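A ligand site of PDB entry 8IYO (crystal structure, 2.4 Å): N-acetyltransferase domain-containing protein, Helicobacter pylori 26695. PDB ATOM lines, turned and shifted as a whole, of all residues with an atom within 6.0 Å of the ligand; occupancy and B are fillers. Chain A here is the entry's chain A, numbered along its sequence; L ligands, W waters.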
ATOM      1  N   ARG A  23     -12.470 -33.650  24.618  1.00  0.00           N
ATOM      2  CA  ARG A  23     -12.061 -32.308  25.003  1.00  0.00           C
ATOM      3  C   ARG A  23     -13.246 -31.518  25.573  1.00  0.00           C
ATOM      4  O   ARG A  23     -13.096 -30.784  26.557  1.00  0.00           O
ATOM      5  CB  ARG A  23     -11.460 -31.557  23.810  1.00  0.00           C
ATOM      6  CG  ARG A  23     -10.162 -32.125  23.198  1.00  0.00           C
ATOM      7  CD  ARG A  23      -9.195 -32.767  24.209  1.00  0.00           C
ATOM      8  NE  ARG A  23      -8.992 -31.945  25.387  1.00  0.00           N
ATOM      9  CZ  ARG A  23      -8.875 -32.430  26.625  1.00  0.00           C
ATOM     10  NH1 ARG A  23      -8.876 -33.736  26.858  1.00  0.00           N
ATOM     11  NH2 ARG A  23      -8.760 -31.582  27.639  1.00  0.00           N
ATOM     12  N   ASN A  27     -14.163 -29.986  29.782  1.00  0.00           N
ATOM     13  CA  ASN A  27     -14.358 -28.554  30.051  1.00  0.00           C
ATOM     14  C   ASN A  27     -15.835 -28.274  30.270  1.00  0.00           C
ATOM     15  O   ASN A  27     -16.479 -27.580  29.467  1.00  0.00           O
ATOM     16  CB  ASN A  27     -13.805 -27.718  28.903  1.00  0.00           C
ATOM     17  CG  ASN A  27     -12.282 -27.766  28.822  1.00  0.00           C
ATOM     18  OD1 ASN A  27     -11.590 -27.141  29.624  1.00  0.00           O
ATOM     19  ND2 ASN A  27     -11.763 -28.513  27.850  1.00  0.00           N
ATOM     20  N   PHE A  31     -18.395 -24.916  27.697  1.00  0.00           N
ATOM     21  CA  PHE A  31     -18.841 -25.343  26.372  1.00  0.00           C
ATOM     22  C   PHE A  31     -20.188 -26.034  26.475  1.00  0.00           C
ATOM     23  O   PHE A  31     -20.526 -26.641  27.486  1.00  0.00           O
ATOM     24  CB  PHE A  31     -17.836 -26.301  25.708  1.00  0.00           C
ATOM     25  CG  PHE A  31     -16.486 -25.698  25.462  1.00  0.00           C
ATOM     26  CD1 PHE A  31     -15.483 -25.809  26.422  1.00  0.00           C
ATOM     27  CD2 PHE A  31     -16.207 -25.037  24.278  1.00  0.00           C
ATOM     28  CE1 PHE A  31     -14.237 -25.255  26.200  1.00  0.00           C
ATOM     29  CE2 PHE A  31     -14.961 -24.482  24.057  1.00  0.00           C
ATOM     30  CZ  PHE A  31     -13.972 -24.596  25.020  1.00  0.00           C
ATOM     31  N   LEU A  80     -10.714 -17.306  15.248  1.00  0.00           N
ATOM     32  CA  LEU A  80     -10.166 -18.517  15.837  1.00  0.00           C
ATOM     33  C   LEU A  80     -11.282 -19.308  16.519  1.00  0.00           C
ATOM     34  O   LEU A  80     -12.161 -18.735  17.160  1.00  0.00           O
ATOM     35  CB  LEU A  80      -9.073 -18.176  16.845  1.00  0.00           C
ATOM     36  CG  LEU A  80      -8.090 -19.266  17.246  1.00  0.00           C
ATOM     37  CD1 LEU A  80      -7.012 -19.446  16.178  1.00  0.00           C
ATOM     38  CD2 LEU A  80      -7.453 -18.958  18.603  1.00  0.00           C
ATOM     39  N   CYS A  81     -11.225 -20.632  16.397  1.00  0.00           N
ATOM     40  CA  CYS A  81     -12.279 -21.473  16.966  1.00  0.00           C
ATOM     41  C   CYS A  81     -11.737 -22.880  17.175  1.00  0.00           C
ATOM     42  O   CYS A  81     -10.714 -23.254  16.596  1.00  0.00           O
ATOM     43  CB  CYS A  81     -13.516 -21.503  16.069  1.00  0.00           C
ATOM     44  SG  CYS A  81     -13.136 -21.948  14.365  1.00  0.00           S
ATOM     45  N   LYS A  82     -12.446 -23.655  17.995  1.00  0.00           N
ATOM     46  CA  LYS A  82     -12.134 -25.073  18.226  1.00  0.00           C
ATOM     47  C   LYS A  82     -10.677 -25.278  18.616  1.00  0.00           C
ATOM     48  O   LYS A  82      -9.996 -26.187  18.134  1.00  0.00           O
ATOM     49  CB  LYS A  82     -12.465 -25.914  16.992  1.00  0.00           C
ATOM     50  CG  LYS A  82     -13.868 -25.757  16.424  1.00  0.00           C
ATOM     51  CD  LYS A  82     -14.936 -25.805  17.495  1.00  0.00           C
ATOM     52  CE  LYS A  82     -16.311 -25.999  16.857  1.00  0.00           C
ATOM     53  NZ  LYS A  82     -17.385 -25.615  17.810  1.00  0.00           N
ATOM     54  N   PHE A  83     -10.179 -24.413  19.487  1.00  0.00           N
ATOM     55  CA  PHE A  83      -8.785 -24.431  19.931  1.00  0.00           C
ATOM     56  C   PHE A  83      -8.688 -25.338  21.154  1.00  0.00           C
ATOM     57  O   PHE A  83      -9.173 -24.981  22.239  1.00  0.00           O
ATOM     58  CB  PHE A  83      -8.341 -23.002  20.215  1.00  0.00           C
ATOM     59  CG  PHE A  83      -6.877 -22.850  20.489  1.00  0.00           C
ATOM     60  CD1 PHE A  83      -5.966 -23.766  20.013  1.00  0.00           C
ATOM     61  CD2 PHE A  83      -6.421 -21.753  21.202  1.00  0.00           C
ATOM     62  CE1 PHE A  83      -4.620 -23.619  20.255  1.00  0.00           C
ATOM     63  CE2 PHE A  83      -5.065 -21.587  21.437  1.00  0.00           C
ATOM     64  CZ  PHE A  83      -4.163 -22.521  20.968  1.00  0.00           C
ATOM     65  N   HIS A  84      -8.076 -26.513  20.995  1.00  0.00           N
ATOM     66  CA  HIS A  84      -8.039 -27.508  22.061  1.00  0.00           C
ATOM     67  C   HIS A  84      -6.734 -28.302  22.018  1.00  0.00           C
ATOM     68  O   HIS A  84      -6.307 -28.743  20.943  1.00  0.00           O
ATOM     69  CB  HIS A  84      -9.212 -28.484  21.952  1.00  0.00           C
ATOM     70  CG  HIS A  84     -10.553 -27.884  22.257  1.00  0.00           C
ATOM     71  ND1 HIS A  84     -11.036 -27.772  23.540  1.00  0.00           N
ATOM     72  CD2 HIS A  84     -11.500 -27.371  21.447  1.00  0.00           C
ATOM     73  CE1 HIS A  84     -12.234 -27.210  23.499  1.00  0.00           C
ATOM     74  NE2 HIS A  84     -12.536 -26.961  22.243  1.00  0.00           N
ATOM     75  N   ILE A  85      -6.143 -28.505  23.192  1.00  0.00           N
ATOM     76  CA  ILE A  85      -5.007 -29.397  23.386  1.00  0.00           C
ATOM     77  C   ILE A  85      -5.396 -30.419  24.439  1.00  0.00           C
ATOM     78  O   ILE A  85      -6.055 -30.090  25.422  1.00  0.00           O
ATOM     79  CB  ILE A  85      -3.740 -28.628  23.833  1.00  0.00           C
ATOM     80  CG1 ILE A  85      -3.286 -27.641  22.748  1.00  0.00           C
ATOM     81  CG2 ILE A  85      -2.610 -29.589  24.226  1.00  0.00           C
ATOM     82  CD1 ILE A  85      -2.500 -28.275  21.615  1.00  0.00           C
ATOM     83  N   ASN A  86      -5.006 -31.679  24.217  1.00  0.00           N
ATOM     84  CA  ASN A  86      -5.320 -32.749  25.152  1.00  0.00           C
ATOM     85  C   ASN A  86      -4.763 -32.445  26.542  1.00  0.00           C
ATOM     86  O   ASN A  86      -3.687 -31.875  26.699  1.00  0.00           O
ATOM     87  CB  ASN A  86      -4.775 -34.074  24.638  1.00  0.00           C
ATOM     88  CG  ASN A  86      -5.060 -35.220  25.581  1.00  0.00           C
ATOM     89  OD1 ASN A  86      -4.343 -35.413  26.577  1.00  0.00           O
ATOM     90  ND2 ASN A  86      -6.089 -35.993  25.292  1.00  0.00           N
ATOM     91  N   TYR A  89      -1.143 -32.964  27.666  1.00  0.00           N
ATOM     92  CA  TYR A  89      -0.145 -32.213  26.927  1.00  0.00           C
ATOM     93  C   TYR A  89      -0.262 -30.705  27.112  1.00  0.00           C
ATOM     94  O   TYR A  89       0.451 -29.940  26.454  1.00  0.00           O
ATOM     95  CB  TYR A  89      -0.226 -32.555  25.434  1.00  0.00           C
ATOM     96  CG  TYR A  89       0.083 -33.996  25.115  1.00  0.00           C
ATOM     97  CD1 TYR A  89      -0.861 -34.988  25.330  1.00  0.00           C
ATOM     98  CD2 TYR A  89       1.325 -34.360  24.595  1.00  0.00           C
ATOM     99  CE1 TYR A  89      -0.580 -36.307  25.042  1.00  0.00           C
ATOM    100  CE2 TYR A  89       1.606 -35.679  24.307  1.00  0.00           C
ATOM    101  CZ  TYR A  89       0.654 -36.652  24.531  1.00  0.00           C
ATOM    102  OH  TYR A  89       0.932 -37.968  24.234  1.00  0.00           O
ATOM    103  N   GLN A  90      -1.156 -30.252  28.002  1.00  0.00           N
ATOM    104  CA  GLN A  90      -1.334 -28.830  28.240  1.00  0.00           C
ATOM    105  C   GLN A  90      -0.203 -28.272  29.106  1.00  0.00           C
ATOM    106  O   GLN A  90       0.492 -29.008  29.812  1.00  0.00           O
ATOM    107  CB  GLN A  90      -2.678 -28.556  28.914  1.00  0.00           C
ATOM    108  CG  GLN A  90      -3.888 -28.618  27.986  1.00  0.00           C
ATOM    109  CD  GLN A  90      -5.206 -28.437  28.729  1.00  0.00           C
ATOM    110  OE1 GLN A  90      -5.220 -28.072  29.906  1.00  0.00           O
ATOM    111  NE2 GLN A  90      -6.313 -28.702  28.051  1.00  0.00           N
ATOM    112  N   SER A  91      -0.014 -26.954  29.018  1.00  0.00           N
ATOM    113  CA  SER A  91       0.913 -26.215  29.868  1.00  0.00           C
ATOM    114  C   SER A  91       2.371 -26.592  29.620  1.00  0.00           C
ATOM    115  O   SER A  91       3.190 -26.548  30.537  1.00  0.00           O
ATOM    116  CB  SER A  91       0.564 -26.389  31.349  1.00  0.00           C
ATOM    117  OG  SER A  91      -0.815 -26.151  31.578  1.00  0.00           O
ATOM    118  N   GLN A  92       2.715 -26.958  28.376  1.00  0.00           N
ATOM    119  CA  GLN A  92       4.091 -27.200  27.980  1.00  0.00           C
ATOM    120  C   GLN A  92       4.574 -26.286  26.871  1.00  0.00           C
ATOM    121  O   GLN A  92       5.732 -26.400  26.455  1.00  0.00           O
ATOM    122  CB  GLN A  92       4.288 -28.651  27.526  1.00  0.00           C
ATOM    123  CG  GLN A  92       3.820 -29.704  28.504  1.00  0.00           C
ATOM    124  CD  GLN A  92       3.950 -31.100  27.935  1.00  0.00           C
ATOM    125  OE1 GLN A  92       4.604 -31.317  26.916  1.00  0.00           O
ATOM    126  NE2 GLN A  92       3.317 -32.073  28.593  1.00  0.00           N
ATOM    127  N   GLY A  93       3.723 -25.407  26.353  1.00  0.00           N
ATOM    128  CA  GLY A  93       4.065 -24.581  25.210  1.00  0.00           C
ATOM    129  C   GLY A  93       3.532 -25.066  23.880  1.00  0.00           C
ATOM    130  O   GLY A  93       3.764 -24.412  22.863  1.00  0.00           O
ATOM    131  N   LEU A  94       2.804 -26.193  23.858  1.00  0.00           N
ATOM    132  CA  LEU A  94       2.335 -26.723  22.580  1.00  0.00           C
ATOM    133  C   LEU A  94       1.182 -25.892  22.026  1.00  0.00           C
ATOM    134  O   LEU A  94       1.119 -25.636  20.821  1.00  0.00           O
ATOM    135  CB  LEU A  94       1.937 -28.189  22.733  1.00  0.00           C
ATOM    136  CG  LEU A  94       3.069 -29.171  23.061  1.00  0.00           C
ATOM    137  CD1 LEU A  94       2.531 -30.580  23.255  1.00  0.00           C
ATOM    138  CD2 LEU A  94       4.151 -29.161  21.995  1.00  0.00           C
ATOM    139  N   GLY A  95       0.260 -25.452  22.886  1.00  0.00           N
ATOM    140  CA  GLY A  95      -0.861 -24.668  22.405  1.00  0.00           C
ATOM    141  C   GLY A  95      -0.433 -23.352  21.779  1.00  0.00           C
ATOM    142  O   GLY A  95      -0.933 -22.953  20.726  1.00  0.00           O
ATOM    143  N   GLN A  96       0.503 -22.648  22.425  1.00  0.00           N
ATOM    144  CA  GLN A  96       1.054 -21.425  21.849  1.00  0.00           C
ATOM    145  C   GLN A  96       1.673 -21.688  20.471  1.00  0.00           C
ATOM    146  O   GLN A  96       1.497 -20.893  19.540  1.00  0.00           O
ATOM    147  CB  GLN A  96       2.088 -20.807  22.778  1.00  0.00           C
ATOM    148  CG  GLN A  96       2.794 -19.601  22.160  1.00  0.00           C
ATOM    149  CD  GLN A  96       3.694 -18.868  23.137  1.00  0.00           C
ATOM    150  OE1 GLN A  96       3.563 -19.007  24.355  1.00  0.00           O
ATOM    151  NE2 GLN A  96       4.610 -18.075  22.605  1.00  0.00           N
ATOM    152  N   LYS A  97       2.404 -22.794  20.334  1.00  0.00           N
ATOM    153  CA  LYS A  97       2.999 -23.111  19.031  1.00  0.00           C
ATOM    154  C   LYS A  97       1.920 -23.408  17.990  1.00  0.00           C
ATOM    155  O   LYS A  97       2.033 -22.977  16.840  1.00  0.00           O
ATOM    156  CB  LYS A  97       3.975 -24.280  19.162  1.00  0.00           C
ATOM    157  CG  LYS A  97       5.339 -23.856  19.676  1.00  0.00           C
ATOM    158  CD  LYS A  97       6.202 -25.030  20.094  1.00  0.00           C
ATOM    159  CE  LYS A  97       7.209 -24.600  21.150  1.00  0.00           C
ATOM    160  NZ  LYS A  97       7.826 -23.287  20.787  1.00  0.00           N
ATOM    161  N   LEU A 116     -12.074 -13.611  18.396  1.00  0.00           N
ATOM    162  CA  LEU A 116     -12.500 -14.831  19.068  1.00  0.00           C
ATOM    163  C   LEU A 116     -13.390 -14.479  20.240  1.00  0.00           C
ATOM    164  O   LEU A 116     -13.474 -13.309  20.657  1.00  0.00           O
ATOM    165  CB  LEU A 116     -11.302 -15.662  19.530  1.00  0.00           C
ATOM    166  CG  LEU A 116     -10.311 -15.044  20.527  1.00  0.00           C
ATOM    167  CD1 LEU A 116     -10.736 -15.256  21.974  1.00  0.00           C
ATOM    168  CD2 LEU A 116      -8.939 -15.665  20.305  1.00  0.00           C
ATOM    169  N   HIS A 117     -14.044 -15.498  20.778  1.00  0.00           N
ATOM    170  CA  HIS A 117     -14.728 -15.390  22.053  1.00  0.00           C
ATOM    171  C   HIS A 117     -14.475 -16.657  22.844  1.00  0.00           C
ATOM    172  O   HIS A 117     -14.222 -17.726  22.280  1.00  0.00           O
ATOM    173  CB  HIS A 117     -16.231 -15.133  21.873  1.00  0.00           C
ATOM    174  CG  HIS A 117     -16.919 -16.125  20.981  1.00  0.00           C
ATOM    175  ND1 HIS A 117     -17.277 -17.386  21.417  1.00  0.00           N
ATOM    176  CD2 HIS A 117     -17.298 -16.042  19.687  1.00  0.00           C
ATOM    177  CE1 HIS A 117     -17.857 -18.039  20.416  1.00  0.00           C
ATOM    178  NE2 HIS A 117     -17.886 -17.247  19.362  1.00  0.00           N
ATOM    179  N   VAL A 118     -14.500 -16.532  24.169  1.00  0.00           N
ATOM    180  CA  VAL A 118     -14.149 -17.631  25.058  1.00  0.00           C
ATOM    181  C   VAL A 118     -14.874 -17.431  26.380  1.00  0.00           C
ATOM    182  O   VAL A 118     -15.063 -16.296  26.827  1.00  0.00           O
ATOM    183  CB  VAL A 118     -12.620 -17.729  25.244  1.00  0.00           C
ATOM    184  CG1 VAL A 118     -12.056 -16.430  25.810  1.00  0.00           C
ATOM    185  CG2 VAL A 118     -12.241 -18.915  26.125  1.00  0.00           C
ATOM    186  N   SER A 119     -15.306 -18.534  26.985  1.00  0.00           N
ATOM    187  CA  SER A 119     -15.929 -18.456  28.309  1.00  0.00           C
ATOM    188  C   SER A 119     -14.902 -18.039  29.343  1.00  0.00           C
ATOM    189  O   SER A 119     -13.737 -18.460  29.290  1.00  0.00           O
ATOM    190  CB  SER A 119     -16.536 -19.805  28.689  1.00  0.00           C
ATOM    191  OG  SER A 119     -17.584 -20.156  27.796  1.00  0.00           O
ATOM    192  N   GLN A 122     -12.516 -20.456  31.159  1.00  0.00           N
ATOM    193  CA  GLN A 122     -11.330 -21.030  30.502  1.00  0.00           C
ATOM    194  C   GLN A 122     -10.114 -20.180  30.828  1.00  0.00           C
ATOM    195  O   GLN A 122      -9.652 -19.362  30.022  1.00  0.00           O
ATOM    196  CB  GLN A 122     -11.559 -21.135  28.996  1.00  0.00           C
ATOM    197  CG  GLN A 122     -12.789 -21.954  28.607  1.00  0.00           C
ATOM    198  CD  GLN A 122     -12.856 -23.290  29.337  1.00  0.00           C
ATOM    199  OE1 GLN A 122     -13.741 -23.508  30.158  1.00  0.00           O
ATOM    200  NE2 GLN A 122     -11.898 -24.175  29.046  1.00  0.00           N
ATOM    201  N   ILE A 123      -9.552 -20.412  32.012  1.00  0.00           N
ATOM    202  CA  ILE A 123      -8.489 -19.551  32.532  1.00  0.00           C
ATOM    203  C   ILE A 123      -7.238 -19.636  31.668  1.00  0.00           C
ATOM    204  O   ILE A 123      -6.638 -18.620  31.301  1.00  0.00           O
ATOM    205  CB  ILE A 123      -8.176 -19.911  33.999  1.00  0.00           C
ATOM    206  CG1 ILE A 123      -9.438 -19.803  34.864  1.00  0.00           C
ATOM    207  CG2 ILE A 123      -7.063 -19.015  34.539  1.00  0.00           C
ATOM    208  CD1 ILE A 123     -10.093 -18.441  34.827  1.00  0.00           C
ATOM    209  N   LYS A 124      -6.807 -20.865  31.334  1.00  0.00           N
ATOM    210  CA  LYS A 124      -5.585 -21.026  30.539  1.00  0.00           C
ATOM    211  C   LYS A 124      -5.669 -20.286  29.218  1.00  0.00           C
ATOM    212  O   LYS A 124      -4.719 -19.600  28.813  1.00  0.00           O
ATOM    213  CB  LYS A 124      -5.310 -22.513  30.292  1.00  0.00           C
ATOM    214  CG  LYS A 124      -4.927 -23.316  31.522  1.00  0.00           C
ATOM    215  CD  LYS A 124      -4.549 -24.740  31.133  1.00  0.00           C
ATOM    216  CE  LYS A 124      -4.369 -25.622  32.351  1.00  0.00           C
ATOM    217  NZ  LYS A 124      -3.498 -26.785  32.052  1.00  0.00           N
ATOM    218  N   ALA A 125      -6.804 -20.422  28.518  1.00  0.00           N
ATOM    219  CA  ALA A 125      -6.957 -19.759  27.223  1.00  0.00           C
ATOM    220  C   ALA A 125      -6.933 -18.243  27.357  1.00  0.00           C
ATOM    221  O   ALA A 125      -6.311 -17.554  26.544  1.00  0.00           O
ATOM    222  CB  ALA A 125      -8.264 -20.212  26.560  1.00  0.00           C
ATOM    223  N   ASN A 127      -5.411 -16.463  29.664  1.00  0.00           N
ATOM    224  CA  ASN A 127      -4.021 -16.078  29.891  1.00  0.00           C
ATOM    225  C   ASN A 127      -3.201 -16.140  28.601  1.00  0.00           C
ATOM    226  O   ASN A 127      -2.383 -15.248  28.345  1.00  0.00           O
ATOM    227  CB  ASN A 127      -3.397 -16.955  30.965  1.00  0.00           C
ATOM    228  CG  ASN A 127      -3.931 -16.658  32.352  1.00  0.00           C
ATOM    229  OD1 ASN A 127      -4.520 -15.600  32.584  1.00  0.00           O
ATOM    230  ND2 ASN A 127      -3.725 -17.580  33.283  1.00  0.00           N
ATOM    231  N   LEU A 128      -3.408 -17.169  27.782  1.00  0.00           N
ATOM    232  CA  LEU A 128      -2.639 -17.298  26.539  1.00  0.00           C
ATOM    233  C   LEU A 128      -2.953 -16.157  25.588  1.00  0.00           C
ATOM    234  O   LEU A 128      -2.049 -15.542  25.005  1.00  0.00           O
ATOM    235  CB  LEU A 128      -2.914 -18.652  25.876  1.00  0.00           C
ATOM    236  CG  LEU A 128      -2.310 -18.862  24.477  1.00  0.00           C
ATOM    237  CD1 LEU A 128      -0.801 -18.598  24.468  1.00  0.00           C
ATOM    238  CD2 LEU A 128      -2.610 -20.248  23.932  1.00  0.00           C
ATOM    239  N   TYR A 129      -4.252 -15.846  25.409  1.00  0.00           N
ATOM    240  CA  TYR A 129      -4.628 -14.787  24.481  1.00  0.00           C
ATOM    241  C   TYR A 129      -4.072 -13.440  24.923  1.00  0.00           C
ATOM    242  O   TYR A 129      -3.692 -12.617  24.088  1.00  0.00           O
ATOM    243  CB  TYR A 129      -6.153 -14.724  24.348  1.00  0.00           C
ATOM    244  CG  TYR A 129      -6.808 -15.992  23.821  1.00  0.00           C
ATOM    245  CD1 TYR A 129      -6.159 -16.798  22.888  1.00  0.00           C
ATOM    246  CD2 TYR A 129      -8.066 -16.381  24.261  1.00  0.00           C
ATOM    247  CE1 TYR A 129      -6.755 -17.964  22.403  1.00  0.00           C
ATOM    248  CE2 TYR A 129      -8.661 -17.537  23.790  1.00  0.00           C
ATOM    249  CZ  TYR A 129      -8.006 -18.322  22.863  1.00  0.00           C
ATOM    250  OH  TYR A 129      -8.622 -19.475  22.399  1.00  0.00           O
ATOM    251  N   LYS A 131      -1.234 -13.171  26.603  1.00  0.00           N
ATOM    252  CA  LYS A 131       0.182 -13.262  26.295  1.00  0.00           C
ATOM    253  C   LYS A 131       0.458 -13.042  24.819  1.00  0.00           C
ATOM    254  O   LYS A 131       1.484 -12.447  24.447  1.00  0.00           O
ATOM    255  CB  LYS A 131       0.735 -14.615  26.742  1.00  0.00           C
ATOM    256  CG  LYS A 131       2.234 -14.738  26.574  1.00  0.00           C
ATOM    257  CD  LYS A 131       2.675 -16.194  26.575  1.00  0.00           C
ATOM    258  CE  LYS A 131       4.170 -16.286  26.287  1.00  0.00           C
ATOM    259  NZ  LYS A 131       4.700 -17.667  26.465  1.00  0.00           N
HETATM  260  N1  LIG L   1      -2.286 -21.897  34.476  1.00  0.00           N
HETATM  261  C1  LIG L   1      -2.353 -20.649  33.987  1.00  0.00           C
HETATM  262  N2  LIG L   1      -2.082 -20.220  32.755  1.00  0.00           N
HETATM  263  C2  LIG L   1      -1.690 -21.221  31.962  1.00  0.00           C
HETATM  264  C3  LIG L   1      -1.569 -22.550  32.317  1.00  0.00           C
HETATM  265  C4  LIG L   1      -1.881 -22.891  33.649  1.00  0.00           C
HETATM  266  N3  LIG L   1      -1.815 -24.140  34.139  1.00  0.00           N
HETATM  267  N4  LIG L   1      -1.133 -23.307  31.235  1.00  0.00           N
HETATM  268  C5  LIG L   1      -1.015 -22.436  30.265  1.00  0.00           C
HETATM  269  N5  LIG L   1      -1.345 -21.152  30.632  1.00  0.00           N
HETATM  270  C6  LIG L   1      -1.286 -19.952  29.800  1.00  0.00           C
HETATM  271  C7  LIG L   1      -0.063 -19.080  30.110  1.00  0.00           C
HETATM  272  O1  LIG L   1      -0.310 -17.745  29.696  1.00  0.00           O
HETATM  273  C8  LIG L   1       0.948 -19.739  29.187  1.00  0.00           C
HETATM  274  O2  LIG L   1       2.098 -18.899  28.955  1.00  0.00           O
HETATM  275  P1  LIG L   1       3.440 -19.135  29.734  1.00  0.00           P
HETATM  276  O3  LIG L   1       3.840 -20.559  29.527  1.00  0.00           O
HETATM  277  O4  LIG L   1       3.161 -18.811  31.220  1.00  0.00           O
HETATM  278  O5  LIG L   1       4.474 -18.139  29.195  1.00  0.00           O
HETATM  279  C9  LIG L   1       0.122 -19.892  27.922  1.00  0.00           C
HETATM  280  O6  LIG L   1      -1.148 -20.357  28.438  1.00  0.00           O
HETATM  281  C10 LIG L   1       0.656 -20.865  26.909  1.00  0.00           C
HETATM  282  O7  LIG L   1       0.557 -22.193  27.453  1.00  0.00           O
HETATM  283  P2  LIG L   1       0.657 -23.473  26.537  1.00  0.00           P
HETATM  284  O8  LIG L   1       1.331 -24.590  27.222  1.00  0.00           O
HETATM  285  O9  LIG L   1       1.261 -23.094  25.186  1.00  0.00           O
HETATM  286  O10 LIG L   1      -0.846 -23.800  26.278  1.00  0.00           O
HETATM  287  P3  LIG L   1      -1.735 -25.109  26.161  1.00  0.00           P
HETATM  288  O11 LIG L   1      -0.886 -26.235  25.705  1.00  0.00           O
HETATM  289  O12 LIG L   1      -2.421 -25.305  27.516  1.00  0.00           O
HETATM  290  O13 LIG L   1      -2.802 -24.721  25.044  1.00  0.00           O
HETATM  291  C11 LIG L   1      -5.129 -24.291  25.332  1.00  0.00           C
HETATM  292  C12 LIG L   1      -3.715 -23.743  25.555  1.00  0.00           C
HETATM  293  C13 LIG L   1      -6.140 -23.167  25.605  1.00  0.00           C
HETATM  294  C14 LIG L   1      -5.265 -24.761  23.886  1.00  0.00           C
HETATM  295  C15 LIG L   1      -5.372 -25.485  26.289  1.00  0.00           C
HETATM  296  O14 LIG L   1      -4.949 -25.180  27.610  1.00  0.00           O
HETATM  297  C16 LIG L   1      -6.796 -26.013  26.309  1.00  0.00           C
HETATM  298  O15 LIG L   1      -7.104 -26.943  25.567  1.00  0.00           O
HETATM  299  N6  LIG L   1      -7.665 -25.432  27.149  1.00  0.00           N
HETATM  300  C17 LIG L   1      -9.056 -25.844  27.267  1.00  0.00           C
HETATM  301  C18 LIG L   1      -9.835 -25.593  25.990  1.00  0.00           C
HETATM  302  C19 LIG L   1     -10.072 -24.119  25.746  1.00  0.00           C
HETATM  303  O16 LIG L   1     -10.328 -23.347  26.668  1.00  0.00           O
HETATM  304  N7  LIG L   1      -9.995 -23.736  24.478  1.00  0.00           N
HETATM  305  C20 LIG L   1     -10.213 -22.360  24.059  1.00  0.00           C
HETATM  306  C21 LIG L   1     -11.592 -22.168  23.464  1.00  0.00           C
HETATM  307  S1  LIG L   1     -11.717 -20.468  22.835  1.00  0.00           S
HETATM  308  C22 LIG L   1     -11.382 -20.720  21.115  1.00  0.00           C
HETATM  309  O17 LIG L   1     -11.325 -21.807  20.615  1.00  0.00           O
HETATM  310  C23 LIG L   1     -11.170 -19.434  20.367  1.00  0.00           C
HETATM  311  O   HOH W   1      -8.549 -22.905  28.910  1.00  0.00           O
HETATM  312  O   HOH W   2       1.569 -21.315  32.288  1.00  0.00           O
HETATM  313  O   HOH W   3       1.341 -27.607  26.201  1.00  0.00           O
HETATM  314  O   HOH W   4     -14.497 -22.375  20.056  1.00  0.00           O
HETATM  315  O   HOH W   5      -9.386 -28.890  25.642  1.00  0.00           O
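Water W1 bridges an oxygen (O16) of the ligand (2.9 Å) and the backbone NH of Ala 125 (3.1 Å). Water W5 lies within hydrogen-bond range of a ring nitrogen (ND1) of His 84 (2.9 Å), an oxygen (O15) of the ligand (3.0 Å), the guanidinium group (NE) of Arg 23 (3.1 Å) and the side-chain amide nitrogen (ND2) of Asn 27 (3.3 Å). Water W4 bridges N of Lys 82 and O17 of the ligand.
The side-chain amide oxygen (OE1) of Gln 96 sits at hydrogen-bond distance from the side-chain amino group (NZ) of Lys 131, at 2.7 Å. The side-chain hydroxyl of Ser 91 is in hydrogen-bond range of the side-chain amino group of Lys 124 (2.8 Å). The side-chain amide oxygen (OD1) of Asn 27 lies within hydrogen-bond range of the side-chain amide nitrogen (NE2) of Gln 122. The backbone carbonyl oxygen (O) of Ile 85 is in hydrogen-bond range of the side-chain amide nitrogen (NE2) of Gln 90 (3.0 Å). NE of Arg 23 sits at hydrogen-bond distance from O of Ile 85 (3.5 Å). The side-chain amide oxygen (OE1) of Gln 90 sits at hydrogen-bond distance from the side-chain amino group (NZ) of Lys 124, at 3.0 Å. The backbone carbonyl oxygen (O) of Arg 23 lies within hydrogen-bond range of the side-chain amide nitrogen (ND2) of Asn 27 (2.9 Å).
A sulfur (S1) of the ligand lies close to the backbone carbonyl oxygen (O) of His 117, at 3.8 Å. Asn 27 touches the ligand. CZ of Phe 31 touches C21 of the ligand, 3.7 Å away. Leu 80 touches the ligand. C of Cys 81 touches O17 of the ligand, at 3.6 Å. ND1 of His 84 touches C18 of the ligand, 3.5 Å away. Leu 94 touches the ligand (N to O9, 3.7 Å). CB of Leu 116 touches C23 of the ligand, at 3.9 Å. Val 118 touches the ligand (CG2 to S1, 3.7 Å). Lys 124 touches the ligand (CE to N3, 3.5 Å). Ala 125 touches the ligand. CB of Leu 128 touches O6 of the ligand, at 3.5 Å. Hydrophobic or aromatic side chains that line the ligand: Phe 31, Phe 83, His 84, Ile 85, Leu 116, Val 118, Ala 125 and Leu 128. Within 4 Å of the ligand: Asn 27, Phe 31, Leu 80, Cys 81, Lys 82, Phe 83, His 84, Ile 85, Gln 90, Ser 91, Gln 92, Gly 93, Leu 94, Gly 95, Gln 96, Leu 116, His 117, Val 118, Gln 122, Lys 124, Ala 125, Asn 127, Leu 128, Tyr 129 and Lys 131.
O8 of the ligand lies within hydrogen-bond range of N of Gly 93 (2.7 Å). An oxygen (O17) of the ligand lies within hydrogen-bond range of the backbone NH of Phe 83 (3.1 Å). The backbone carbonyl oxygen of Phe 83 is in hydrogen-bond range of a nitrogen (N7) of the ligand, at 2.7 Å. NZ of Lys 131 lies within salt-bridge range of O5 of the ligand, 2.8 Å away. The backbone NH (N) of Ser 91 lies close to an oxygen (O8) of the ligand, at 3.3 Å. OG of Ser 91 lies within hydrogen-bond range of N4 of the ligand, at 2.9 Å. N of Gln 96 lies within hydrogen-bond range of O9 of the ligand (2.9 Å). The side-chain amide nitrogen (NE2) of Gln 122 sits at hydrogen-bond distance from an oxygen (O16) of the ligand (3.0 Å). N of Gln 92 lies within hydrogen-bond range of O8 of the ligand. The backbone NH (N) of Ile 85 lies within hydrogen-bond range of an oxygen (O15) of the ligand, 3.0 Å away. O11 of the ligand sits at hydrogen-bond distance from N of Gly 95 (3.1 Å). O15 of the ligand sits at hydrogen-bond distance from NE2 of Gln 90, 3.1 Å away. A nitrogen (N2) of the ligand lies within hydrogen-bond range of the side-chain amide nitrogen of Asn 127, at 3.2 Å. The side-chain hydroxyl of Tyr 129 lies close to a sulfur (S1) of the ligand, at 3.3 Å. O17 of the ligand is in hydrogen-bond range of N of Lys 82.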
